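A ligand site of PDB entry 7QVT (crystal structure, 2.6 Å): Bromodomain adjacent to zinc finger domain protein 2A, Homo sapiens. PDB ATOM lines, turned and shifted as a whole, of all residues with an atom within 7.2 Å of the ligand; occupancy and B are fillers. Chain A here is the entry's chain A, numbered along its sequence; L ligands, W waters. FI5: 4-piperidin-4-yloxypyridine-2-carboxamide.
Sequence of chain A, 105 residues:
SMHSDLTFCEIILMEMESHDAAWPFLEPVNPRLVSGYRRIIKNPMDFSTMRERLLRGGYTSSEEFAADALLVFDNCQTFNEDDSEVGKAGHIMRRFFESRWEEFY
Merely in contact with the ligand: Phe 25 (3.6 Å), Val 29 (3.97 Å), Val 34 (3.3 Å), Tyr 37 (3.8 Å), Phe 79 (3.5 Å) and Val 86 (3.7 Å). Of the 22 residues printed, 8 come within 4 Å of the ligand.
Water W1 lies within hydrogen-bond range of O03 of the ligand, OH of Tyr 37, O of Asn 75 and N of Cys 76. Water W2 bridges O of Val 72 (3.1 Å) and N01 of the ligand (3.2 Å).
O of Cys 76 sits at hydrogen-bond distance from ND2 of Asn 80, at 3.2 Å. The side-chain sulfur of Cys 76 sits at hydrogen-bond distance from the backbone carbonyl oxygen of Val 86 (3.7 Å).
The backbone carbonyl oxygen of Pro 24 is in hydrogen-bond range of a nitrogen (N01) of the ligand, 3.0 Å away. O03 of the ligand is in hydrogen-bond range of ND2 of Asn 80 (2.9 Å).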
ATOM      1  N   TRP A  23     -31.003 -16.057 -28.055  1.00  0.00           N
ATOM      2  CA  TRP A  23     -29.943 -15.344 -28.763  1.00  0.00           C
ATOM      3  C   TRP A  23     -28.646 -15.183 -27.980  1.00  0.00           C
ATOM      4  O   TRP A  23     -27.574 -15.325 -28.603  1.00  0.00           O
ATOM      5  CB  TRP A  23     -30.470 -13.982 -29.256  1.00  0.00           C
ATOM      6  CG  TRP A  23     -31.115 -13.162 -28.222  1.00  0.00           C
ATOM      7  CD1 TRP A  23     -32.419 -13.218 -27.821  1.00  0.00           C
ATOM      8  CD2 TRP A  23     -30.508 -12.126 -27.450  1.00  0.00           C
ATOM      9  NE1 TRP A  23     -32.653 -12.277 -26.844  1.00  0.00           N
ATOM     10  CE2 TRP A  23     -31.498 -11.596 -26.594  1.00  0.00           C
ATOM     11  CE3 TRP A  23     -29.209 -11.598 -27.389  1.00  0.00           C
ATOM     12  CZ2 TRP A  23     -31.235 -10.572 -25.687  1.00  0.00           C
ATOM     13  CZ3 TRP A  23     -28.946 -10.567 -26.501  1.00  0.00           C
ATOM     14  CH2 TRP A  23     -29.953 -10.068 -25.655  1.00  0.00           C
ATOM     15  N   PRO A  24     -28.623 -14.929 -26.664  1.00  0.00           N
ATOM     16  CA  PRO A  24     -27.314 -14.751 -25.991  1.00  0.00           C
ATOM     17  C   PRO A  24     -26.522 -16.035 -25.864  1.00  0.00           C
ATOM     18  O   PRO A  24     -25.374 -15.987 -25.402  1.00  0.00           O
ATOM     19  CB  PRO A  24     -27.689 -14.193 -24.614  1.00  0.00           C
ATOM     20  CG  PRO A  24     -29.135 -13.834 -24.685  1.00  0.00           C
ATOM     21  CD  PRO A  24     -29.715 -14.779 -25.690  1.00  0.00           C
ATOM     22  N   PHE A  25     -27.078 -17.188 -26.263  1.00  0.00           N
ATOM     23  CA  PHE A  25     -26.472 -18.476 -25.967  1.00  0.00           C
ATOM     24  C   PHE A  25     -26.249 -19.343 -27.204  1.00  0.00           C
ATOM     25  O   PHE A  25     -25.893 -20.515 -27.058  1.00  0.00           O
ATOM     26  CB  PHE A  25     -27.335 -19.236 -24.950  1.00  0.00           C
ATOM     27  CG  PHE A  25     -27.917 -18.352 -23.894  1.00  0.00           C
ATOM     28  CD1 PHE A  25     -27.098 -17.722 -22.974  1.00  0.00           C
ATOM     29  CD2 PHE A  25     -29.284 -18.105 -23.856  1.00  0.00           C
ATOM     30  CE1 PHE A  25     -27.632 -16.887 -22.009  1.00  0.00           C
ATOM     31  CE2 PHE A  25     -29.827 -17.280 -22.895  1.00  0.00           C
ATOM     32  CZ  PHE A  25     -28.997 -16.658 -21.977  1.00  0.00           C
ATOM     33  N   LEU A  26     -26.424 -18.793 -28.412  1.00  0.00           N
ATOM     34  CA  LEU A  26     -26.367 -19.614 -29.622  1.00  0.00           C
ATOM     35  C   LEU A  26     -24.930 -19.954 -29.996  1.00  0.00           C
ATOM     36  O   LEU A  26     -24.653 -21.067 -30.441  1.00  0.00           O
ATOM     37  CB  LEU A  26     -27.066 -18.893 -30.769  1.00  0.00           C
ATOM     38  CG  LEU A  26     -28.592 -18.860 -30.685  1.00  0.00           C
ATOM     39  CD1 LEU A  26     -29.117 -17.845 -31.662  1.00  0.00           C
ATOM     40  CD2 LEU A  26     -29.177 -20.239 -30.960  1.00  0.00           C
ATOM     41  N   GLU A  27     -24.012 -19.006 -29.835  1.00  0.00           N
ATOM     42  CA  GLU A  27     -22.605 -19.183 -30.135  1.00  0.00           C
ATOM     43  C   GLU A  27     -21.768 -18.700 -28.958  1.00  0.00           C
ATOM     44  O   GLU A  27     -22.261 -17.921 -28.127  1.00  0.00           O
ATOM     45  CB  GLU A  27     -22.198 -18.417 -31.400  1.00  0.00           C
ATOM     46  CG  GLU A  27     -23.032 -18.732 -32.637  1.00  0.00           C
ATOM     47  CD  GLU A  27     -22.996 -17.592 -33.629  1.00  0.00           C
ATOM     48  OE1 GLU A  27     -22.835 -16.434 -33.194  1.00  0.00           O
ATOM     49  OE2 GLU A  27     -23.122 -17.857 -34.854  1.00  0.00           O
ATOM     50  N   VAL A  29     -19.403 -16.755 -26.358  1.00  0.00           N
ATOM     51  CA  VAL A  29     -19.143 -15.345 -26.103  1.00  0.00           C
ATOM     52  C   VAL A  29     -17.757 -14.997 -26.618  1.00  0.00           C
ATOM     53  O   VAL A  29     -16.754 -15.618 -26.240  1.00  0.00           O
ATOM     54  CB  VAL A  29     -19.294 -15.020 -24.614  1.00  0.00           C
ATOM     55  CG1 VAL A  29     -18.824 -13.603 -24.337  1.00  0.00           C
ATOM     56  CG2 VAL A  29     -20.746 -15.211 -24.183  1.00  0.00           C
ATOM     57  N   LEU A  33     -15.179  -8.815 -27.503  1.00  0.00           N
ATOM     58  CA  LEU A  33     -16.280  -7.858 -27.526  1.00  0.00           C
ATOM     59  C   LEU A  33     -16.955  -7.680 -26.167  1.00  0.00           C
ATOM     60  O   LEU A  33     -17.718  -6.732 -26.006  1.00  0.00           O
ATOM     61  CB  LEU A  33     -17.330  -8.275 -28.564  1.00  0.00           C
ATOM     62  CG  LEU A  33     -16.793  -8.472 -29.981  1.00  0.00           C
ATOM     63  CD1 LEU A  33     -17.646  -9.474 -30.750  1.00  0.00           C
ATOM     64  CD2 LEU A  33     -16.715  -7.142 -30.731  1.00  0.00           C
ATOM     65  N   VAL A  34     -16.696  -8.558 -25.217  1.00  0.00           N
ATOM     66  CA  VAL A  34     -17.390  -8.551 -23.925  1.00  0.00           C
ATOM     67  C   VAL A  34     -16.322  -8.399 -22.848  1.00  0.00           C
ATOM     68  O   VAL A  34     -15.733  -9.389 -22.401  1.00  0.00           O
ATOM     69  CB  VAL A  34     -18.223  -9.813 -23.716  1.00  0.00           C
ATOM     70  CG1 VAL A  34     -18.828  -9.821 -22.314  1.00  0.00           C
ATOM     71  CG2 VAL A  34     -19.309  -9.897 -24.780  1.00  0.00           C
ATOM     72  N   SER A  35     -16.067  -7.173 -22.422  1.00  0.00           N
ATOM     73  CA  SER A  35     -14.983  -6.947 -21.469  1.00  0.00           C
ATOM     74  C   SER A  35     -15.327  -7.572 -20.126  1.00  0.00           C
ATOM     75  O   SER A  35     -16.466  -7.505 -19.654  1.00  0.00           O
ATOM     76  CB  SER A  35     -14.680  -5.446 -21.311  1.00  0.00           C
ATOM     77  OG  SER A  35     -15.850  -4.656 -21.431  1.00  0.00           O
ATOM     78  N   TYR A  37     -15.363 -10.800 -19.520  1.00  0.00           N
ATOM     79  CA  TYR A  37     -15.895 -12.160 -19.610  1.00  0.00           C
ATOM     80  C   TYR A  37     -14.800 -13.207 -19.384  1.00  0.00           C
ATOM     81  O   TYR A  37     -15.050 -14.228 -18.731  1.00  0.00           O
ATOM     82  CB  TYR A  37     -16.573 -12.398 -20.959  1.00  0.00           C
ATOM     83  CG  TYR A  37     -17.577 -13.532 -20.907  1.00  0.00           C
ATOM     84  CD1 TYR A  37     -18.853 -13.334 -20.370  1.00  0.00           C
ATOM     85  CD2 TYR A  37     -17.252 -14.802 -21.373  1.00  0.00           C
ATOM     86  CE1 TYR A  37     -19.768 -14.366 -20.306  1.00  0.00           C
ATOM     87  CE2 TYR A  37     -18.166 -15.844 -21.312  1.00  0.00           C
ATOM     88  CZ  TYR A  37     -19.424 -15.621 -20.777  1.00  0.00           C
ATOM     89  OH  TYR A  37     -20.342 -16.635 -20.707  1.00  0.00           O
ATOM     90  N   ILE A  41     -15.817 -15.721 -16.208  1.00  0.00           N
ATOM     91  CA  ILE A  41     -16.357 -17.031 -16.544  1.00  0.00           C
ATOM     92  C   ILE A  41     -15.198 -17.992 -16.775  1.00  0.00           C
ATOM     93  O   ILE A  41     -14.477 -17.875 -17.763  1.00  0.00           O
ATOM     94  CB  ILE A  41     -17.285 -16.962 -17.758  1.00  0.00           C
ATOM     95  CG1 ILE A  41     -18.445 -16.007 -17.477  1.00  0.00           C
ATOM     96  CG2 ILE A  41     -17.795 -18.352 -18.132  1.00  0.00           C
ATOM     97  CD1 ILE A  41     -19.231 -16.341 -16.213  1.00  0.00           C
ATOM     98  N   MET A  45     -19.745 -21.908 -21.922  1.00  0.00           N
ATOM     99  CA  MET A  45     -20.569 -22.945 -22.513  1.00  0.00           C
ATOM    100  C   MET A  45     -21.688 -22.263 -23.281  1.00  0.00           C
ATOM    101  O   MET A  45     -22.132 -21.165 -22.914  1.00  0.00           O
ATOM    102  CB  MET A  45     -21.120 -23.903 -21.458  1.00  0.00           C
ATOM    103  CG  MET A  45     -21.886 -25.109 -22.000  1.00  0.00           C
ATOM    104  SD  MET A  45     -21.023 -26.017 -23.297  1.00  0.00           S
ATOM    105  CE  MET A  45     -19.474 -26.410 -22.478  1.00  0.00           C
ATOM    106  N   VAL A  72     -24.560 -23.163 -18.863  1.00  0.00           N
ATOM    107  CA  VAL A  72     -24.899 -21.978 -19.647  1.00  0.00           C
ATOM    108  C   VAL A  72     -25.601 -20.952 -18.776  1.00  0.00           C
ATOM    109  O   VAL A  72     -25.279 -19.759 -18.804  1.00  0.00           O
ATOM    110  CB  VAL A  72     -25.755 -22.365 -20.866  1.00  0.00           C
ATOM    111  CG1 VAL A  72     -26.130 -21.117 -21.662  1.00  0.00           C
ATOM    112  CG2 VAL A  72     -25.045 -23.362 -21.759  1.00  0.00           C
ATOM    113  N   ASN A  75     -23.405 -19.496 -15.821  1.00  0.00           N
ATOM    114  CA  ASN A  75     -22.518 -18.452 -16.344  1.00  0.00           C
ATOM    115  C   ASN A  75     -23.295 -17.170 -16.620  1.00  0.00           C
ATOM    116  O   ASN A  75     -22.810 -16.073 -16.333  1.00  0.00           O
ATOM    117  CB  ASN A  75     -21.804 -18.921 -17.611  1.00  0.00           C
ATOM    118  CG  ASN A  75     -20.840 -20.068 -17.354  1.00  0.00           C
ATOM    119  OD1 ASN A  75     -20.247 -20.175 -16.276  1.00  0.00           O
ATOM    120  ND2 ASN A  75     -20.674 -20.940 -18.340  1.00  0.00           N
ATOM    121  N   CYS A  76     -24.502 -17.298 -17.182  1.00  0.00           N
ATOM    122  CA  CYS A  76     -25.297 -16.114 -17.490  1.00  0.00           C
ATOM    123  C   CYS A  76     -25.595 -15.307 -16.230  1.00  0.00           C
ATOM    124  O   CYS A  76     -25.418 -14.084 -16.205  1.00  0.00           O
ATOM    125  CB  CYS A  76     -26.592 -16.504 -18.191  1.00  0.00           C
ATOM    126  SG  CYS A  76     -27.693 -15.092 -18.527  1.00  0.00           S
ATOM    127  N   GLN A  77     -26.046 -15.977 -15.175  1.00  0.00           N
ATOM    128  CA  GLN A  77     -26.342 -15.280 -13.931  1.00  0.00           C
ATOM    129  C   GLN A  77     -25.071 -14.757 -13.259  1.00  0.00           C
ATOM    130  O   GLN A  77     -25.107 -13.683 -12.640  1.00  0.00           O
ATOM    131  CB  GLN A  77     -27.096 -16.187 -12.973  1.00  0.00           C
ATOM    132  CG  GLN A  77     -28.543 -16.382 -13.323  1.00  0.00           C
ATOM    133  CD  GLN A  77     -29.100 -17.622 -12.699  1.00  0.00           C
ATOM    134  OE1 GLN A  77     -29.881 -17.552 -11.754  1.00  0.00           O
ATOM    135  NE2 GLN A  77     -28.687 -18.774 -13.199  1.00  0.00           N
ATOM    136  N   PHE A  79     -22.440 -13.543 -14.812  1.00  0.00           N
ATOM    137  CA  PHE A  79     -21.921 -12.391 -15.539  1.00  0.00           C
ATOM    138  C   PHE A  79     -22.924 -11.270 -15.731  1.00  0.00           C
ATOM    139  O   PHE A  79     -22.528 -10.104 -15.747  1.00  0.00           O
ATOM    140  CB  PHE A  79     -21.391 -12.804 -16.913  1.00  0.00           C
ATOM    141  CG  PHE A  79     -20.675 -11.706 -17.628  1.00  0.00           C
ATOM    142  CD1 PHE A  79     -19.377 -11.346 -17.253  1.00  0.00           C
ATOM    143  CD2 PHE A  79     -21.296 -10.998 -18.643  1.00  0.00           C
ATOM    144  CE1 PHE A  79     -18.727 -10.316 -17.885  1.00  0.00           C
ATOM    145  CE2 PHE A  79     -20.635  -9.963 -19.284  1.00  0.00           C
ATOM    146  CZ  PHE A  79     -19.345  -9.626 -18.906  1.00  0.00           C
ATOM    147  N   ASN A  80     -24.204 -11.571 -15.896  1.00  0.00           N
ATOM    148  CA  ASN A  80     -25.182 -10.550 -16.226  1.00  0.00           C
ATOM    149  C   ASN A  80     -26.130 -10.307 -15.064  1.00  0.00           C
ATOM    150  O   ASN A  80     -26.521 -11.245 -14.362  1.00  0.00           O
ATOM    151  CB  ASN A  80     -25.948 -10.933 -17.486  1.00  0.00           C
ATOM    152  CG  ASN A  80     -25.025 -11.217 -18.660  1.00  0.00           C
ATOM    153  OD1 ASN A  80     -24.563 -10.293 -19.326  1.00  0.00           O
ATOM    154  ND2 ASN A  80     -24.737 -12.494 -18.896  1.00  0.00           N
ATOM    155  N   SER A  84     -30.660  -7.144 -16.548  1.00  0.00           N
ATOM    156  CA  SER A  84     -30.096  -6.886 -17.856  1.00  0.00           C
ATOM    157  C   SER A  84     -30.862  -7.673 -18.924  1.00  0.00           C
ATOM    158  O   SER A  84     -31.538  -8.659 -18.625  1.00  0.00           O
ATOM    159  CB  SER A  84     -28.614  -7.254 -17.903  1.00  0.00           C
ATOM    160  OG  SER A  84     -28.452  -8.652 -17.852  1.00  0.00           O
ATOM    161  N   GLU A  85     -30.734  -7.220 -20.176  1.00  0.00           N
ATOM    162  CA  GLU A  85     -31.402  -7.886 -21.287  1.00  0.00           C
ATOM    163  C   GLU A  85     -30.956  -9.339 -21.414  1.00  0.00           C
ATOM    164  O   GLU A  85     -31.788 -10.245 -21.572  1.00  0.00           O
ATOM    165  CB  GLU A  85     -31.153  -7.134 -22.599  1.00  0.00           C
ATOM    166  CG  GLU A  85     -31.972  -5.869 -22.743  1.00  0.00           C
ATOM    167  CD  GLU A  85     -33.468  -6.128 -22.599  1.00  0.00           C
ATOM    168  OE1 GLU A  85     -34.036  -6.864 -23.429  1.00  0.00           O
ATOM    169  OE2 GLU A  85     -34.069  -5.597 -21.639  1.00  0.00           O
ATOM    170  N   VAL A  86     -29.643  -9.585 -21.346  1.00  0.00           N
ATOM    171  CA  VAL A  86     -29.148 -10.963 -21.395  1.00  0.00           C
ATOM    172  C   VAL A  86     -29.632 -11.744 -20.176  1.00  0.00           C
ATOM    173  O   VAL A  86     -30.045 -12.903 -20.283  1.00  0.00           O
ATOM    174  CB  VAL A  86     -27.613 -10.976 -21.503  1.00  0.00           C
ATOM    175  CG1 VAL A  86     -27.062 -12.384 -21.278  1.00  0.00           C
ATOM    176  CG2 VAL A  86     -27.167 -10.447 -22.869  1.00  0.00           C
ATOM    177  N   GLY A  87     -29.596 -11.113 -18.997  1.00  0.00           N
ATOM    178  CA  GLY A  87     -30.083 -11.774 -17.791  1.00  0.00           C
ATOM    179  C   GLY A  87     -31.532 -12.210 -17.895  1.00  0.00           C
ATOM    180  O   GLY A  87     -31.885 -13.320 -17.492  1.00  0.00           O
HETATM  181  C16 FI5 L   1     -23.932  -8.027 -22.824  1.00  0.00           C
HETATM  182  C15 FI5 L   1     -24.367  -6.667 -23.372  1.00  0.00           C
HETATM  183  C13 FI5 L   1     -22.087  -5.801 -23.046  1.00  0.00           C
HETATM  184  C12 FI5 L   1     -21.652  -7.164 -22.490  1.00  0.00           C
HETATM  185  C11 FI5 L   1     -22.480  -8.275 -23.021  1.00  0.00           C
HETATM  186  C02 FI5 L   1     -23.887 -14.048 -22.050  1.00  0.00           C
HETATM  187  C04 FI5 L   1     -23.674 -12.748 -22.822  1.00  0.00           C
HETATM  188  C06 FI5 L   1     -23.979 -11.553 -24.773  1.00  0.00           C
HETATM  189  C07 FI5 L   1     -23.309 -10.466 -24.227  1.00  0.00           C
HETATM  190  C08 FI5 L   1     -22.807 -10.537 -22.937  1.00  0.00           C
HETATM  191  C09 FI5 L   1     -22.992 -11.714 -22.209  1.00  0.00           C
HETATM  192  N01 FI5 L   1     -24.592 -15.155 -22.676  1.00  0.00           N
HETATM  193  N05 FI5 L   1     -24.141 -12.650 -24.050  1.00  0.00           N
HETATM  194  N14 FI5 L   1     -23.538  -5.565 -22.843  1.00  0.00           N
HETATM  195  O03 FI5 L   1     -23.486 -14.156 -20.940  1.00  0.00           O
HETATM  196  O10 FI5 L   1     -22.118  -9.455 -22.372  1.00  0.00           O
HETATM  197  O   HOH W   1     -22.554 -16.096 -19.714  1.00  0.00           O
HETATM  198  O   HOH W   2     -24.199 -17.747 -20.894  1.00  0.00           O
